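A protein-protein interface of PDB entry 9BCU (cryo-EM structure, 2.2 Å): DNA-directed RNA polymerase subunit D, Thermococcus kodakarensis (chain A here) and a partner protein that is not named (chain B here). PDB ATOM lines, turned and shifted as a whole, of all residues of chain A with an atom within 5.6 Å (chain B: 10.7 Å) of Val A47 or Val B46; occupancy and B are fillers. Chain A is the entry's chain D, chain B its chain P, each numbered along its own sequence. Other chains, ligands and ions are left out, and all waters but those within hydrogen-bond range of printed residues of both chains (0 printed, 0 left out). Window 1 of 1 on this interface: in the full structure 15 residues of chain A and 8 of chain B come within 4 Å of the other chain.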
ATOM      1  N   VAL A  44      -0.680 -24.832 -18.076  1.00  0.00           N
ATOM      2  CA  VAL A  44       0.066 -23.951 -17.186  1.00  0.00           C
ATOM      3  C   VAL A  44       0.444 -22.681 -17.934  1.00  0.00           C
ATOM      4  O   VAL A  44       1.056 -22.730 -19.008  1.00  0.00           O
ATOM      5  CB  VAL A  44       1.308 -24.668 -16.637  1.00  0.00           C
ATOM      6  CG1 VAL A  44       2.229 -23.681 -15.943  1.00  0.00           C
ATOM      7  CG2 VAL A  44       0.900 -25.781 -15.686  1.00  0.00           C
ATOM      8  N   ASP A  45       0.078 -21.534 -17.367  1.00  0.00           N
ATOM      9  CA  ASP A  45       0.342 -20.234 -17.973  1.00  0.00           C
ATOM     10  C   ASP A  45       1.432 -19.445 -17.266  1.00  0.00           C
ATOM     11  O   ASP A  45       2.221 -18.768 -17.928  1.00  0.00           O
ATOM     12  CB  ASP A  45      -0.943 -19.398 -18.005  1.00  0.00           C
ATOM     13  CG  ASP A  45      -0.853 -18.227 -18.961  1.00  0.00           C
ATOM     14  OD1 ASP A  45      -0.306 -18.404 -20.071  1.00  0.00           O
ATOM     15  OD2 ASP A  45      -1.329 -17.129 -18.606  1.00  0.00           O
ATOM     16  N   GLU A  46       1.497 -19.511 -15.938  1.00  0.00           N
ATOM     17  CA  GLU A  46       2.494 -18.781 -15.172  1.00  0.00           C
ATOM     18  C   GLU A  46       3.026 -19.670 -14.059  1.00  0.00           C
ATOM     19  O   GLU A  46       2.261 -20.381 -13.403  1.00  0.00           O
ATOM     20  CB  GLU A  46       1.910 -17.491 -14.580  1.00  0.00           C
ATOM     21  CG  GLU A  46       2.953 -16.513 -14.069  1.00  0.00           C
ATOM     22  CD  GLU A  46       2.726 -15.102 -14.573  1.00  0.00           C
ATOM     23  OE1 GLU A  46       1.561 -14.652 -14.577  1.00  0.00           O
ATOM     24  OE2 GLU A  46       3.712 -14.443 -14.965  1.00  0.00           O
ATOM     25  N   VAL A  47       4.340 -19.628 -13.854  1.00  0.00           N
ATOM     26  CA  VAL A  47       5.011 -20.413 -12.824  1.00  0.00           C
ATOM     27  C   VAL A  47       5.736 -19.459 -11.887  1.00  0.00           C
ATOM     28  O   VAL A  47       6.493 -18.592 -12.339  1.00  0.00           O
ATOM     29  CB  VAL A  47       5.996 -21.431 -13.429  1.00  0.00           C
ATOM     30  CG1 VAL A  47       6.511 -22.371 -12.351  1.00  0.00           C
ATOM     31  CG2 VAL A  47       5.338 -22.212 -14.553  1.00  0.00           C
ATOM     32  N   GLU A  48       5.506 -19.620 -10.586  1.00  0.00           N
ATOM     33  CA  GLU A  48       6.205 -18.857  -9.559  1.00  0.00           C
ATOM     34  C   GLU A  48       7.309 -19.740  -8.989  1.00  0.00           C
ATOM     35  O   GLU A  48       7.030 -20.736  -8.316  1.00  0.00           O
ATOM     36  CB  GLU A  48       5.243 -18.399  -8.465  1.00  0.00           C
ATOM     37  CG  GLU A  48       5.928 -17.784  -7.257  1.00  0.00           C
ATOM     38  CD  GLU A  48       4.946 -17.364  -6.181  1.00  0.00           C
ATOM     39  OE1 GLU A  48       4.441 -16.223  -6.249  1.00  0.00           O
ATOM     40  OE2 GLU A  48       4.679 -18.173  -5.269  1.00  0.00           O
ATOM     41  N   PHE A  49       8.560 -19.370  -9.253  1.00  0.00           N
ATOM     42  CA  PHE A  49       9.704 -20.190  -8.879  1.00  0.00           C
ATOM     43  C   PHE A  49      10.262 -19.743  -7.534  1.00  0.00           C
ATOM     44  O   PHE A  49      10.556 -18.559  -7.339  1.00  0.00           O
ATOM     45  CB  PHE A  49      10.793 -20.113  -9.949  1.00  0.00           C
ATOM     46  CG  PHE A  49      10.596 -21.075 -11.085  1.00  0.00           C
ATOM     47  CD1 PHE A  49      10.921 -22.414 -10.941  1.00  0.00           C
ATOM     48  CD2 PHE A  49      10.088 -20.640 -12.297  1.00  0.00           C
ATOM     49  CE1 PHE A  49      10.741 -23.300 -11.985  1.00  0.00           C
ATOM     50  CE2 PHE A  49       9.906 -21.521 -13.345  1.00  0.00           C
ATOM     51  CZ  PHE A  49      10.233 -22.853 -13.188  1.00  0.00           C
ATOM     52  N   ASP A  58      14.776 -21.404 -15.759  1.00  0.00           N
ATOM     53  CA  ASP A  58      13.400 -21.232 -15.303  1.00  0.00           C
ATOM     54  C   ASP A  58      12.428 -21.200 -16.475  1.00  0.00           C
ATOM     55  O   ASP A  58      11.340 -21.785 -16.405  1.00  0.00           O
ATOM     56  CB  ASP A  58      13.279 -19.954 -14.473  1.00  0.00           C
ATOM     57  CG  ASP A  58      13.743 -20.142 -13.042  1.00  0.00           C
ATOM     58  OD1 ASP A  58      14.238 -21.241 -12.716  1.00  0.00           O
ATOM     59  OD2 ASP A  58      13.613 -19.190 -12.245  1.00  0.00           O
ATOM     60  N   GLU A  59      12.802 -20.518 -17.561  1.00  0.00           N
ATOM     61  CA  GLU A  59      11.932 -20.441 -18.730  1.00  0.00           C
ATOM     62  C   GLU A  59      11.744 -21.810 -19.377  1.00  0.00           C
ATOM     63  O   GLU A  59      10.636 -22.152 -19.805  1.00  0.00           O
ATOM     64  CB  GLU A  59      12.495 -19.441 -19.740  1.00  0.00           C
ATOM     65  CG  GLU A  59      14.002 -19.523 -19.928  1.00  0.00           C
ATOM     66  CD  GLU A  59      14.749 -18.478 -19.122  1.00  0.00           C
ATOM     67  OE1 GLU A  59      14.292 -18.145 -18.009  1.00  0.00           O
ATOM     68  OE2 GLU A  59      15.794 -17.991 -19.603  1.00  0.00           O
ATOM     69  N   ALA A  62       9.425 -23.833 -17.162  1.00  0.00           N
ATOM     70  CA  ALA A  62       8.060 -23.331 -17.296  1.00  0.00           C
ATOM     71  C   ALA A  62       7.433 -23.767 -18.615  1.00  0.00           C
ATOM     72  O   ALA A  62       6.257 -24.148 -18.655  1.00  0.00           O
ATOM     73  CB  ALA A  62       8.047 -21.807 -17.173  1.00  0.00           C
ATOM     74  N   LEU A  65       6.552 -27.399 -18.363  1.00  0.00           N
ATOM     75  CA  LEU A  65       5.332 -27.543 -17.579  1.00  0.00           C
ATOM     76  C   LEU A  65       4.100 -27.149 -18.382  1.00  0.00           C
ATOM     77  O   LEU A  65       3.028 -27.738 -18.201  1.00  0.00           O
ATOM     78  CB  LEU A  65       5.421 -26.703 -16.306  1.00  0.00           C
ATOM     79  CG  LEU A  65       6.360 -27.211 -15.212  1.00  0.00           C
ATOM     80  CD1 LEU A  65       6.878 -26.047 -14.384  1.00  0.00           C
ATOM     81  CD2 LEU A  65       5.661 -28.231 -14.330  1.00  0.00           C
ATOM     82  N   PHE A 133       8.470 -24.818  -6.855  1.00  0.00           N
ATOM     83  CA  PHE A 133       7.744 -23.797  -7.597  1.00  0.00           C
ATOM     84  C   PHE A 133       6.250 -24.001  -7.398  1.00  0.00           C
ATOM     85  O   PHE A 133       5.800 -25.042  -6.913  1.00  0.00           O
ATOM     86  CB  PHE A 133       8.102 -23.819  -9.089  1.00  0.00           C
ATOM     87  CG  PHE A 133       7.845 -25.141  -9.762  1.00  0.00           C
ATOM     88  CD1 PHE A 133       6.600 -25.433 -10.300  1.00  0.00           C
ATOM     89  CD2 PHE A 133       8.852 -26.082  -9.873  1.00  0.00           C
ATOM     90  CE1 PHE A 133       6.364 -26.645 -10.917  1.00  0.00           C
ATOM     91  CE2 PHE A 133       8.622 -27.292 -10.495  1.00  0.00           C
ATOM     92  CZ  PHE A 133       7.377 -27.574 -11.017  1.00  0.00           C
ATOM     93  N   ASN A 134       5.485 -22.982  -7.784  1.00  0.00           N
ATOM     94  CA  ASN A 134       4.030 -23.048  -7.839  1.00  0.00           C
ATOM     95  C   ASN A 134       3.597 -22.722  -9.261  1.00  0.00           C
ATOM     96  O   ASN A 134       3.896 -21.636  -9.768  1.00  0.00           O
ATOM     97  CB  ASN A 134       3.393 -22.077  -6.842  1.00  0.00           C
ATOM     98  CG  ASN A 134       3.586 -22.507  -5.403  1.00  0.00           C
ATOM     99  OD1 ASN A 134       2.972 -23.470  -4.944  1.00  0.00           O
ATOM    100  ND2 ASN A 134       4.441 -21.793  -4.681  1.00  0.00           N
ATOM    101  N   ALA A 135       2.897 -23.656  -9.897  1.00  0.00           N
ATOM    102  CA  ALA A 135       2.460 -23.509 -11.278  1.00  0.00           C
ATOM    103  C   ALA A 135       0.968 -23.213 -11.313  1.00  0.00           C
ATOM    104  O   ALA A 135       0.172 -23.945 -10.717  1.00  0.00           O
ATOM    105  CB  ALA A 135       2.770 -24.771 -12.088  1.00  0.00           C
ATOM    106  N   TYR A 136       0.596 -22.146 -12.013  1.00  0.00           N
ATOM    107  CA  TYR A 136      -0.790 -21.714 -12.126  1.00  0.00           C
ATOM    108  C   TYR A 136      -1.317 -22.062 -13.510  1.00  0.00           C
ATOM    109  O   TYR A 136      -0.684 -21.737 -14.520  1.00  0.00           O
ATOM    110  CB  TYR A 136      -0.915 -20.212 -11.867  1.00  0.00           C
ATOM    111  CG  TYR A 136      -0.268 -19.767 -10.575  1.00  0.00           C
ATOM    112  CD1 TYR A 136      -0.829 -20.091  -9.348  1.00  0.00           C
ATOM    113  CD2 TYR A 136       0.907 -19.028 -10.584  1.00  0.00           C
ATOM    114  CE1 TYR A 136      -0.241 -19.689  -8.165  1.00  0.00           C
ATOM    115  CE2 TYR A 136       1.504 -18.621  -9.406  1.00  0.00           C
ATOM    116  CZ  TYR A 136       0.925 -18.954  -8.199  1.00  0.00           C
ATOM    117  OH  TYR A 136       1.514 -18.551  -7.023  1.00  0.00           O
ATOM    118  N   VAL B  42      13.742 -15.288  -2.473  1.00  0.00           N
ATOM    119  CA  VAL B  42      12.469 -14.680  -2.843  1.00  0.00           C
ATOM    120  C   VAL B  42      11.920 -15.331  -4.111  1.00  0.00           C
ATOM    121  O   VAL B  42      12.654 -15.887  -4.936  1.00  0.00           O
ATOM    122  CB  VAL B  42      12.626 -13.161  -3.021  1.00  0.00           C
ATOM    123  CG1 VAL B  42      13.102 -12.528  -1.723  1.00  0.00           C
ATOM    124  CG2 VAL B  42      13.599 -12.858  -4.150  1.00  0.00           C
ATOM    125  N   ALA B  43      10.601 -15.261  -4.259  1.00  0.00           N
ATOM    126  CA  ALA B  43       9.914 -15.871  -5.387  1.00  0.00           C
ATOM    127  C   ALA B  43       9.912 -14.940  -6.594  1.00  0.00           C
ATOM    128  O   ALA B  43       9.883 -13.713  -6.460  1.00  0.00           O
ATOM    129  CB  ALA B  43       8.478 -16.235  -5.011  1.00  0.00           C
ATOM    130  N   ARG B  44       9.946 -15.542  -7.780  1.00  0.00           N
ATOM    131  CA  ARG B  44       9.907 -14.812  -9.037  1.00  0.00           C
ATOM    132  C   ARG B  44       8.862 -15.434  -9.952  1.00  0.00           C
ATOM    133  O   ARG B  44       8.631 -16.646  -9.924  1.00  0.00           O
ATOM    134  CB  ARG B  44      11.277 -14.808  -9.730  1.00  0.00           C
ATOM    135  CG  ARG B  44      11.863 -16.192  -9.950  1.00  0.00           C
ATOM    136  CD  ARG B  44      13.232 -16.326  -9.310  1.00  0.00           C
ATOM    137  NE  ARG B  44      13.921 -17.533  -9.748  1.00  0.00           N
ATOM    138  CZ  ARG B  44      14.439 -18.439  -8.932  1.00  0.00           C
ATOM    139  NH1 ARG B  44      14.370 -18.304  -7.617  1.00  0.00           N
ATOM    140  NH2 ARG B  44      15.042 -19.508  -9.445  1.00  0.00           N
ATOM    141  N   ARG B  45       8.229 -14.591 -10.763  1.00  0.00           N
ATOM    142  CA  ARG B  45       7.186 -15.021 -11.685  1.00  0.00           C
ATOM    143  C   ARG B  45       7.783 -15.175 -13.078  1.00  0.00           C
ATOM    144  O   ARG B  45       8.355 -14.223 -13.621  1.00  0.00           O
ATOM    145  CB  ARG B  45       6.028 -14.023 -11.704  1.00  0.00           C
ATOM    146  CG  ARG B  45       5.290 -13.903 -10.382  1.00  0.00           C
ATOM    147  CD  ARG B  45       4.462 -15.144 -10.099  1.00  0.00           C
ATOM    148  NE  ARG B  45       3.104 -15.024 -10.613  1.00  0.00           N
ATOM    149  CZ  ARG B  45       2.012 -15.055  -9.861  1.00  0.00           C
ATOM    150  NH1 ARG B  45       2.082 -15.200  -8.548  1.00  0.00           N
ATOM    151  NH2 ARG B  45       0.821 -14.938 -10.441  1.00  0.00           N
ATOM    152  N   VAL B  46       7.650 -16.367 -13.651  1.00  0.00           N
ATOM    153  CA  VAL B  46       8.161 -16.674 -14.981  1.00  0.00           C
ATOM    154  C   VAL B  46       6.993 -17.106 -15.854  1.00  0.00           C
ATOM    155  O   VAL B  46       6.253 -18.030 -15.500  1.00  0.00           O
ATOM    156  CB  VAL B  46       9.244 -17.770 -14.937  1.00  0.00           C
ATOM    157  CG1 VAL B  46       9.728 -18.094 -16.340  1.00  0.00           C
ATOM    158  CG2 VAL B  46      10.403 -17.335 -14.055  1.00  0.00           C
ATOM    159  N   LYS B  47       6.828 -16.435 -16.992  1.00  0.00           N
ATOM    160  CA  LYS B  47       5.763 -16.786 -17.919  1.00  0.00           C
ATOM    161  C   LYS B  47       6.092 -18.085 -18.643  1.00  0.00           C
ATOM    162  O   LYS B  47       7.219 -18.292 -19.103  1.00  0.00           O
ATOM    163  CB  LYS B  47       5.544 -15.660 -18.929  1.00  0.00           C
ATOM    164  CG  LYS B  47       4.740 -14.491 -18.390  1.00  0.00           C
ATOM    165  CD  LYS B  47       4.995 -13.227 -19.195  1.00  0.00           C
ATOM    166  CE  LYS B  47       4.519 -13.382 -20.629  1.00  0.00           C
ATOM    167  NZ  LYS B  47       5.589 -13.045 -21.608  1.00  0.00           N
ATOM    168  N   ALA B  48       5.098 -18.965 -18.744  1.00  0.00           N
ATOM    169  CA  ALA B  48       5.259 -20.246 -19.429  1.00  0.00           C
ATOM    170  C   ALA B  48       5.124 -20.005 -20.926  1.00  0.00           C
ATOM    171  O   ALA B  48       4.043 -20.139 -21.506  1.00  0.00           O
ATOM    172  CB  ALA B  48       4.238 -21.259 -18.929  1.00  0.00           C
ATOM    173  N   ILE B  49       6.245 -19.646 -21.552  1.00  0.00           N
ATOM    174  CA  ILE B  49       6.323 -19.331 -22.980  1.00  0.00           C
ATOM    175  C   ILE B  49       5.338 -18.229 -23.360  1.00  0.00           C
ATOM    176  O   ILE B  49       4.273 -18.497 -23.916  1.00  0.00           O
ATOM    177  CB  ILE B  49       6.095 -20.588 -23.846  1.00  0.00           C
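O of Arg B44 sits at hydrogen-bond distance from N of Phe A49, at 2.8 Å.
The guanidinium group (NE) of Arg B44 lies within salt-bridge range of the side-chain carboxylate (OD2) of Asp A58 (3.0 Å).
NH1 of Arg B45 is in salt-bridge range of OE1 of Glu A48 (3.4 Å).
O of Val A47 lies within hydrogen-bond range of N of Val B46, 2.8 Å away.
The backbone NH (N) of Ala B48 sits at hydrogen-bond distance from the backbone carbonyl oxygen (O) of Asp A45.
The backbone carbonyl oxygen of Tyr A136 is in hydrogen-bond range of the backbone NH of Asp A45 (3.0 Å).
O of Glu A46 lies within hydrogen-bond range of N of Tyr A136 (2.8 Å).
O of Asn A134 is in hydrogen-bond range of N of Glu A48 (2.7 Å).
Among the printed residues, pairs that only touch across the chains: Glu A48 with Arg B44 (3.3 Å), Phe A49 with Ala B43 (3.4 Å), Val A44 with Ala B48 (3.5 Å), Ala A62 with Ala B48 (3.5 Å), Tyr A136 with Arg B45 (3.6 Å), Glu A46 with Lys B47 (3.6 Å), Val A47 with Arg B45 (3.7 Å), Glu A48 with Ala B43 (3.7 Å), Phe A49 with Val B46 (3.8 Å), Glu A46 with Arg B45 (3.8 Å), Val A47 with Arg B44 (3.8 Å), Glu A46 with Val B46 (3.8 Å), Asp A58 with Val B46 (3.9 Å) and Asp A45 with Lys B47 (3.995 Å).
Of chain B, only Arg B44 (3.8 Å), Arg B45 (3.7 Å) and Val B46 (2.8 Å) come within 4 Å of Val A47.
Of chain B, only Arg B45 (3.8 Å), Val B46 (3.8 Å) and Lys B47 (3.6 Å) come within 4 Å of Glu A46.
Printed residues of chain B within 4 Å of Phe A49: Ala B43 (3.4 Å), Arg B44 (2.8 Å) and Val B46 (3.8 Å).
No residue of chain B comes within 4 Å of Phe A133.
Of the printed residues of chain B, Val A44 touches Ala B48 (3.5 Å).
Of the printed residues of chain A, Arg B44 touches Val A47, Glu A48, Phe A49 and Asp A58.
The nearest printed residue of chain A that does not touch Val B46 is Glu A59 (4.01 Å).
The nearest printed residue of chain B that does not touch Glu A48 is Val B46 (5.0 Å).
Hydrophobic or aromatic side chains of chain A within 4 Å of the printed part of chain B: Val A47, Phe A49, Ala A62 and Tyr A136.
Of the 8 printed residues of chain B, 6 touch a printed residue of chain A.
Among the printed residues, 19 pairs touch across the chains.
Among the printed residues, Asp or Glu carboxylates within 4 Å of a Lys or Arg side-chain nitrogen of the other chain: Glu A48 with Arg B45 and Asp A58 with Arg B44.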
